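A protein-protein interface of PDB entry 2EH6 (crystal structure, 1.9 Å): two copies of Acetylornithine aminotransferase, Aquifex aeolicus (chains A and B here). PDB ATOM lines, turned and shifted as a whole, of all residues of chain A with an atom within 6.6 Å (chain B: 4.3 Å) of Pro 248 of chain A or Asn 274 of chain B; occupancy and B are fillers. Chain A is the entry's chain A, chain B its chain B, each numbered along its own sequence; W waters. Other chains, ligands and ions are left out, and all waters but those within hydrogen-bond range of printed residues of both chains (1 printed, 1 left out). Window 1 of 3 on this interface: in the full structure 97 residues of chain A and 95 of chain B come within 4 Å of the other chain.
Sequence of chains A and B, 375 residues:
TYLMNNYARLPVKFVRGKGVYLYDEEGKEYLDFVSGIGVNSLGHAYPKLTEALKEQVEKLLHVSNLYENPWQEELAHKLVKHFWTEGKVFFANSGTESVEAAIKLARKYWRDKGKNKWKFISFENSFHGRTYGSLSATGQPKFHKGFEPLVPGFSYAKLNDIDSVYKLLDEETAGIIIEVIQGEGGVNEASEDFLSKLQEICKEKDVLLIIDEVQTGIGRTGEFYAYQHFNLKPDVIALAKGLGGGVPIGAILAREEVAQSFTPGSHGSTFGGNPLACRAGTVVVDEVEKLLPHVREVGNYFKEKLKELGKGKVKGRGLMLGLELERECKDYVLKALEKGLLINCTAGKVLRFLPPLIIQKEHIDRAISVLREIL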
ATOM      1  N   ALA A  92     -12.950  -2.231   0.842  1.00  0.00           N
ATOM      2  CA  ALA A  92     -12.430  -3.512   0.383  1.00  0.00           C
ATOM      3  C   ALA A  92     -11.217  -3.873   1.254  1.00  0.00           C
ATOM      4  O   ALA A  92     -11.023  -3.283   2.320  1.00  0.00           O
ATOM      5  CB  ALA A  92     -12.028  -3.419  -1.089  1.00  0.00           C
ATOM      6  N   ASN A  93     -10.389  -4.810   0.803  1.00  0.00           N
ATOM      7  CA  ASN A  93      -9.238  -5.217   1.616  1.00  0.00           C
ATOM      8  C   ASN A  93      -7.897  -4.977   0.966  1.00  0.00           C
ATOM      9  O   ASN A  93      -6.860  -5.187   1.594  1.00  0.00           O
ATOM     10  CB  ASN A  93      -9.343  -6.702   1.952  1.00  0.00           C
ATOM     11  CG  ASN A  93     -10.612  -7.034   2.679  1.00  0.00           C
ATOM     12  OD1 ASN A  93     -10.735  -6.785   3.879  1.00  0.00           O
ATOM     13  ND2 ASN A  93     -11.583  -7.585   1.952  1.00  0.00           N
ATOM     14  N   SER A  94      -7.910  -4.539  -0.284  1.00  0.00           N
ATOM     15  CA  SER A  94      -6.668  -4.326  -1.004  1.00  0.00           C
ATOM     16  C   SER A  94      -6.864  -3.348  -2.131  1.00  0.00           C
ATOM     17  O   SER A  94      -7.993  -2.970  -2.452  1.00  0.00           O
ATOM     18  CB  SER A  94      -6.185  -5.647  -1.602  1.00  0.00           C
ATOM     19  OG  SER A  94      -7.151  -6.150  -2.524  1.00  0.00           O
ATOM     20  N   LYS A 241      -3.208   0.563   0.347  1.00  0.00           N
ATOM     21  CA  LYS A 241      -1.861   0.693   0.880  1.00  0.00           C
ATOM     22  C   LYS A 241      -1.765   1.590   2.121  1.00  0.00           C
ATOM     23  O   LYS A 241      -2.244   1.223   3.199  1.00  0.00           O
ATOM     24  CB  LYS A 241      -0.908   1.181  -0.220  1.00  0.00           C
ATOM     25  CG  LYS A 241      -0.682   0.138  -1.330  1.00  0.00           C
ATOM     26  CD  LYS A 241       0.567   0.419  -2.154  1.00  0.00           C
ATOM     27  CE  LYS A 241       0.932  -0.773  -3.060  1.00  0.00           C
ATOM     28  NZ  LYS A 241       0.100  -0.729  -4.285  1.00  0.00           N
ATOM     29  N   GLY A 244      -4.194   2.226   5.549  1.00  0.00           N
ATOM     30  CA  GLY A 244      -4.272   1.446   6.767  1.00  0.00           C
ATOM     31  C   GLY A 244      -3.015   1.457   7.623  1.00  0.00           C
ATOM     32  O   GLY A 244      -2.982   0.814   8.664  1.00  0.00           O
ATOM     33  N   GLY A 246      -0.476  -0.130   7.517  1.00  0.00           N
ATOM     34  CA  GLY A 246       0.084  -1.449   7.755  1.00  0.00           C
ATOM     35  C   GLY A 246      -1.002  -2.500   7.828  1.00  0.00           C
ATOM     36  O   GLY A 246      -0.757  -3.674   7.549  1.00  0.00           O
ATOM     37  N   VAL A 247      -2.202  -2.085   8.225  1.00  0.00           N
ATOM     38  CA  VAL A 247      -3.338  -3.002   8.305  1.00  0.00           C
ATOM     39  C   VAL A 247      -3.987  -3.045   6.912  1.00  0.00           C
ATOM     40  O   VAL A 247      -4.192  -1.999   6.290  1.00  0.00           O
ATOM     41  CB  VAL A 247      -4.368  -2.502   9.344  1.00  0.00           C
ATOM     42  CG1 VAL A 247      -5.577  -3.441   9.387  1.00  0.00           C
ATOM     43  CG2 VAL A 247      -3.710  -2.417  10.727  1.00  0.00           C
ATOM     44  N   PRO A 248      -4.308  -4.252   6.397  1.00  0.00           N
ATOM     45  CA  PRO A 248      -4.925  -4.353   5.067  1.00  0.00           C
ATOM     46  C   PRO A 248      -6.258  -3.626   4.973  1.00  0.00           C
ATOM     47  O   PRO A 248      -7.148  -3.832   5.795  1.00  0.00           O
ATOM     48  CB  PRO A 248      -5.098  -5.855   4.868  1.00  0.00           C
ATOM     49  CG  PRO A 248      -3.999  -6.450   5.747  1.00  0.00           C
ATOM     50  CD  PRO A 248      -4.083  -5.591   6.973  1.00  0.00           C
ATOM     51  N   ILE A 249      -6.388  -2.778   3.962  1.00  0.00           N
ATOM     52  CA  ILE A 249      -7.624  -2.035   3.755  1.00  0.00           C
ATOM     53  C   ILE A 249      -7.617  -1.467   2.346  1.00  0.00           C
ATOM     54  O   ILE A 249      -6.562  -1.230   1.760  1.00  0.00           O
ATOM     55  CB  ILE A 249      -7.770  -0.879   4.786  1.00  0.00           C
ATOM     56  CG1 ILE A 249      -9.162  -0.242   4.676  1.00  0.00           C
ATOM     57  CG2 ILE A 249      -6.684   0.166   4.556  1.00  0.00           C
ATOM     58  CD1 ILE A 249      -9.473   0.775   5.790  1.00  0.00           C
ATOM     59  N   GLY A 250      -8.807  -1.263   1.796  1.00  0.00           N
ATOM     60  CA  GLY A 250      -8.914  -0.708   0.466  1.00  0.00           C
ATOM     61  C   GLY A 250     -10.262  -0.022   0.378  1.00  0.00           C
ATOM     62  O   GLY A 250     -11.109  -0.199   1.250  1.00  0.00           O
ATOM     63  N   ASN A 274     -14.033  -4.017   8.234  1.00  0.00           N
ATOM     64  CA  ASN A 274     -14.032  -4.586   9.569  1.00  0.00           C
ATOM     65  C   ASN A 274     -13.538  -3.485  10.526  1.00  0.00           C
ATOM     66  O   ASN A 274     -12.852  -2.556  10.111  1.00  0.00           O
ATOM     67  CB  ASN A 274     -13.119  -5.816   9.594  1.00  0.00           C
ATOM     68  CG  ASN A 274     -11.678  -5.462   9.364  1.00  0.00           C
ATOM     69  OD1 ASN A 274     -11.010  -4.950  10.264  1.00  0.00           O
ATOM     70  ND2 ASN A 274     -11.184  -5.713   8.150  1.00  0.00           N
ATOM     71  N   LEU A 276     -11.156  -3.383  12.718  1.00  0.00           N
ATOM     72  CA  LEU A 276      -9.715  -3.249  12.896  1.00  0.00           C
ATOM     73  C   LEU A 276      -9.122  -2.365  11.799  1.00  0.00           C
ATOM     74  O   LEU A 276      -8.335  -1.456  12.069  1.00  0.00           O
ATOM     75  CB  LEU A 276      -9.050  -4.626  12.879  1.00  0.00           C
ATOM     76  CG  LEU A 276      -7.577  -4.643  13.301  1.00  0.00           C
ATOM     77  CD1 LEU A 276      -7.472  -4.252  14.767  1.00  0.00           C
ATOM     78  CD2 LEU A 276      -6.989  -6.024  13.075  1.00  0.00           C
ATOM     79  N   ALA A 277      -9.508  -2.631  10.557  1.00  0.00           N
ATOM     80  CA  ALA A 277      -9.029  -1.858   9.420  1.00  0.00           C
ATOM     81  C   ALA A 277      -9.495  -0.404   9.520  1.00  0.00           C
ATOM     82  O   ALA A 277      -8.740   0.532   9.238  1.00  0.00           O
ATOM     83  CB  ALA A 277      -9.544  -2.479   8.118  1.00  0.00           C
ATOM     84  N   CYS A 278     -10.745  -0.215   9.915  1.00  0.00           N
ATOM     85  CA  CYS A 278     -11.288   1.133  10.030  1.00  0.00           C
ATOM     86  C   CYS A 278     -10.655   1.928  11.169  1.00  0.00           C
ATOM     87  O   CYS A 278     -10.491   3.139  11.066  1.00  0.00           O
ATOM     88  CB  CYS A 278     -12.807   1.074  10.187  1.00  0.00           C
ATOM     89  SG  CYS A 278     -13.671   0.563   8.657  1.00  0.00           S
ATOM     90  N   LEU B  61       3.620  -4.863  11.586  1.00  0.00           N
ATOM     91  CA  LEU B  61       2.348  -5.130  10.924  1.00  0.00           C
ATOM     92  C   LEU B  61       2.511  -5.572   9.478  1.00  0.00           C
ATOM     93  O   LEU B  61       1.763  -6.429   8.992  1.00  0.00           O
ATOM     94  CB  LEU B  61       1.469  -3.871  10.932  1.00  0.00           C
ATOM     95  CG  LEU B  61       0.991  -3.284  12.255  1.00  0.00           C
ATOM     96  CD1 LEU B  61       0.369  -1.923  11.991  1.00  0.00           C
ATOM     97  CD2 LEU B  61      -0.012  -4.226  12.914  1.00  0.00           C
ATOM     98  N   TRP B  71       7.194 -15.753   8.710  1.00  0.00           N
ATOM     99  CA  TRP B  71       5.892 -16.083   9.286  1.00  0.00           C
ATOM    100  C   TRP B  71       4.980 -16.767   8.267  1.00  0.00           C
ATOM    101  O   TRP B  71       4.087 -17.535   8.637  1.00  0.00           O
ATOM    102  CB  TRP B  71       5.240 -14.811   9.826  1.00  0.00           C
ATOM    103  CG  TRP B  71       5.390 -13.638   8.898  1.00  0.00           C
ATOM    104  CD1 TRP B  71       4.575 -13.303   7.850  1.00  0.00           C
ATOM    105  CD2 TRP B  71       6.436 -12.664   8.920  1.00  0.00           C
ATOM    106  NE1 TRP B  71       5.055 -12.178   7.220  1.00  0.00           N
ATOM    107  CE2 TRP B  71       6.196 -11.765   7.856  1.00  0.00           C
ATOM    108  CE3 TRP B  71       7.560 -12.462   9.740  1.00  0.00           C
ATOM    109  CZ2 TRP B  71       7.036 -10.679   7.589  1.00  0.00           C
ATOM    110  CZ3 TRP B  71       8.394 -11.381   9.474  1.00  0.00           C
ATOM    111  CH2 TRP B  71       8.127 -10.503   8.404  1.00  0.00           C
ATOM    112  N   ASN B  93      -5.569 -11.898   0.681  1.00  0.00           N
ATOM    113  CA  ASN B  93      -6.253 -11.157   1.732  1.00  0.00           C
ATOM    114  C   ASN B  93      -7.721 -11.466   1.920  1.00  0.00           C
ATOM    115  O   ASN B  93      -8.342 -10.966   2.857  1.00  0.00           O
ATOM    116  CB  ASN B  93      -6.105  -9.663   1.459  1.00  0.00           C
ATOM    117  CG  ASN B  93      -4.670  -9.239   1.400  1.00  0.00           C
ATOM    118  OD1 ASN B  93      -3.992  -9.179   2.427  1.00  0.00           O
ATOM    119  ND2 ASN B  93      -4.180  -8.961   0.193  1.00  0.00           N
ATOM    120  N   PHE B 271      -0.496  -6.678   0.507  1.00  0.00           N
ATOM    121  CA  PHE B 271      -0.801  -7.045   1.889  1.00  0.00           C
ATOM    122  C   PHE B 271      -0.711  -8.536   2.160  1.00  0.00           C
ATOM    123  O   PHE B 271      -0.615  -8.952   3.314  1.00  0.00           O
ATOM    124  CB  PHE B 271      -2.217  -6.600   2.272  1.00  0.00           C
ATOM    125  CG  PHE B 271      -2.425  -5.117   2.244  1.00  0.00           C
ATOM    126  CD1 PHE B 271      -1.523  -4.259   2.865  1.00  0.00           C
ATOM    127  CD2 PHE B 271      -3.548  -4.577   1.623  1.00  0.00           C
ATOM    128  CE1 PHE B 271      -1.738  -2.882   2.868  1.00  0.00           C
ATOM    129  CE2 PHE B 271      -3.772  -3.199   1.622  1.00  0.00           C
ATOM    130  CZ  PHE B 271      -2.867  -2.352   2.244  1.00  0.00           C
ATOM    131  N   GLY B 272      -0.759  -9.337   1.100  1.00  0.00           N
ATOM    132  CA  GLY B 272      -0.730 -10.781   1.257  1.00  0.00           C
ATOM    133  C   GLY B 272       0.353 -11.364   2.150  1.00  0.00           C
ATOM    134  O   GLY B 272       1.538 -11.086   1.969  1.00  0.00           O
ATOM    135  N   GLY B 273      -0.066 -12.175   3.117  1.00  0.00           N
ATOM    136  CA  GLY B 273       0.879 -12.816   4.019  1.00  0.00           C
ATOM    137  C   GLY B 273       1.596 -11.905   5.000  1.00  0.00           C
ATOM    138  O   GLY B 273       2.696 -12.230   5.460  1.00  0.00           O
ATOM    139  N   ASN B 274       0.987 -10.774   5.340  1.00  0.00           N
ATOM    140  CA  ASN B 274       1.618  -9.857   6.287  1.00  0.00           C
ATOM    141  C   ASN B 274       1.748 -10.571   7.635  1.00  0.00           C
ATOM    142  O   ASN B 274       1.028 -11.533   7.908  1.00  0.00           O
ATOM    143  CB  ASN B 274       0.786  -8.578   6.423  1.00  0.00           C
ATOM    144  CG  ASN B 274      -0.582  -8.831   7.009  1.00  0.00           C
ATOM    145  OD1 ASN B 274      -0.720  -9.059   8.206  1.00  0.00           O
ATOM    146  ND2 ASN B 274      -1.607  -8.796   6.163  1.00  0.00           N
ATOM    147  N   PRO B 275       2.655 -10.101   8.503  1.00  0.00           N
ATOM    148  CA  PRO B 275       2.831 -10.755   9.806  1.00  0.00           C
ATOM    149  C   PRO B 275       1.635 -10.779  10.757  1.00  0.00           C
ATOM    150  O   PRO B 275       1.515 -11.684  11.580  1.00  0.00           O
ATOM    151  CB  PRO B 275       4.063 -10.045  10.392  1.00  0.00           C
ATOM    152  CG  PRO B 275       4.036  -8.690   9.736  1.00  0.00           C
ATOM    153  CD  PRO B 275       3.625  -9.003   8.314  1.00  0.00           C
ATOM    154  N   LEU B 276       0.737  -9.807  10.642  1.00  0.00           N
ATOM    155  CA  LEU B 276      -0.425  -9.783  11.516  1.00  0.00           C
ATOM    156  C   LEU B 276      -1.411 -10.898  11.165  1.00  0.00           C
ATOM    157  O   LEU B 276      -1.921 -11.594  12.048  1.00  0.00           O
ATOM    158  CB  LEU B 276      -1.133  -8.430  11.421  1.00  0.00           C
ATOM    159  CG  LEU B 276      -2.219  -8.206  12.473  1.00  0.00           C
ATOM    160  CD1 LEU B 276      -1.572  -8.167  13.874  1.00  0.00           C
ATOM    161  CD2 LEU B 276      -2.941  -6.898  12.187  1.00  0.00           C
ATOM    162  N   ALA B 277      -1.692 -11.052   9.873  1.00  0.00           N
ATOM    163  CA  ALA B 277      -2.619 -12.087   9.419  1.00  0.00           C
ATOM    164  C   ALA B 277      -2.045 -13.478   9.692  1.00  0.00           C
ATOM    165  O   ALA B 277      -2.750 -14.379  10.157  1.00  0.00           O
ATOM    166  CB  ALA B 277      -2.894 -11.919   7.919  1.00  0.00           C
ATOM    167  N   CYS B 278      -0.768 -13.657   9.386  1.00  0.00           N
ATOM    168  CA  CYS B 278      -0.123 -14.946   9.617  1.00  0.00           C
ATOM    169  C   CYS B 278      -0.056 -15.273  11.104  1.00  0.00           C
ATOM    170  O   CYS B 278      -0.162 -16.435  11.495  1.00  0.00           O
ATOM    171  CB  CYS B 278       1.275 -14.956   8.994  1.00  0.00           C
ATOM    172  SG  CYS B 278       1.245 -14.972   7.175  1.00  0.00           S
HETATM  173  O   HOH W   1      -0.384  -5.864   5.149  1.00  0.00           O
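The backbone carbonyl oxygen (O) of Asn 93 of chain A lies within hydrogen-bond range of the backbone NH (N) of Ile 249 of chain A. OD1 of Asn 93 of chain B sits close to O of Phe 271 of chain B (3.5 Å). The backbone carbonyl oxygen (O) of Phe 271 of chain B is in hydrogen-bond range of the side-chain amide nitrogen (ND2) of Asn 274 of chain B. The side-chain amide oxygen (OD1) of Asn 274 of chain B is in hydrogen-bond range of the backbone NH (N) of Leu 276 of chain B. OD1 of Asn 274 of chain B is in hydrogen-bond range of N of Ala 277 of chain B (2.8 Å). The backbone carbonyl oxygen of Asn 274 of chain B sits at hydrogen-bond distance from the side-chain sulfur of Cys 278 of chain B (3.5 Å).
Hydrophobic or aromatic side chains of chain A within 4 Å of the printed part of chain B: Pro 248. Among the printed residues, no Asp or Glu carboxylate lies within 4 Å of a Lys or Arg side-chain nitrogen of the other chain.
Asn 274 of chain B touches one residue of chain A. Of the printed residues of chain B, Ile 249 of chain A touches Phe 271. Of the printed residues of chain A, Phe 271 of chain B touches Asn 93, Lys 241, Pro 248 and Ile 249. Of the printed residues of chain B, Lys 241 of chain A touches Phe 271 (3.5 Å). Printed residues of chain B within 4 Å of Asn 93 of chain A: Phe 271 (3.4 Å). Ala 277 of chain A touches none of the printed residues of chain B. Asn 274 of chain A touches none of the printed residues of chain B.
Positions printed for both chains: 93, 274, 276, 277 and 278. Of the 5 pairs that touch across the chains among the printed residues, none has its exchanged pair printed and touching as well.
Water W1 lies within hydrogen-bond range of O of Gly 246 of chain A (3.3 Å) and ND2 of Asn 274 of chain B (3.3 Å).
Among the printed residues, pairs that only touch across the chains: Asn 93 of chain A with Phe 271 of chain B, Lys 241 of chain A with Phe 271 of chain B, Pro 248 of chain A with Phe 271 of chain B, Pro 248 of chain A with Asn 274 of chain B and Ile 249 of chain A with Phe 271 of chain B.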
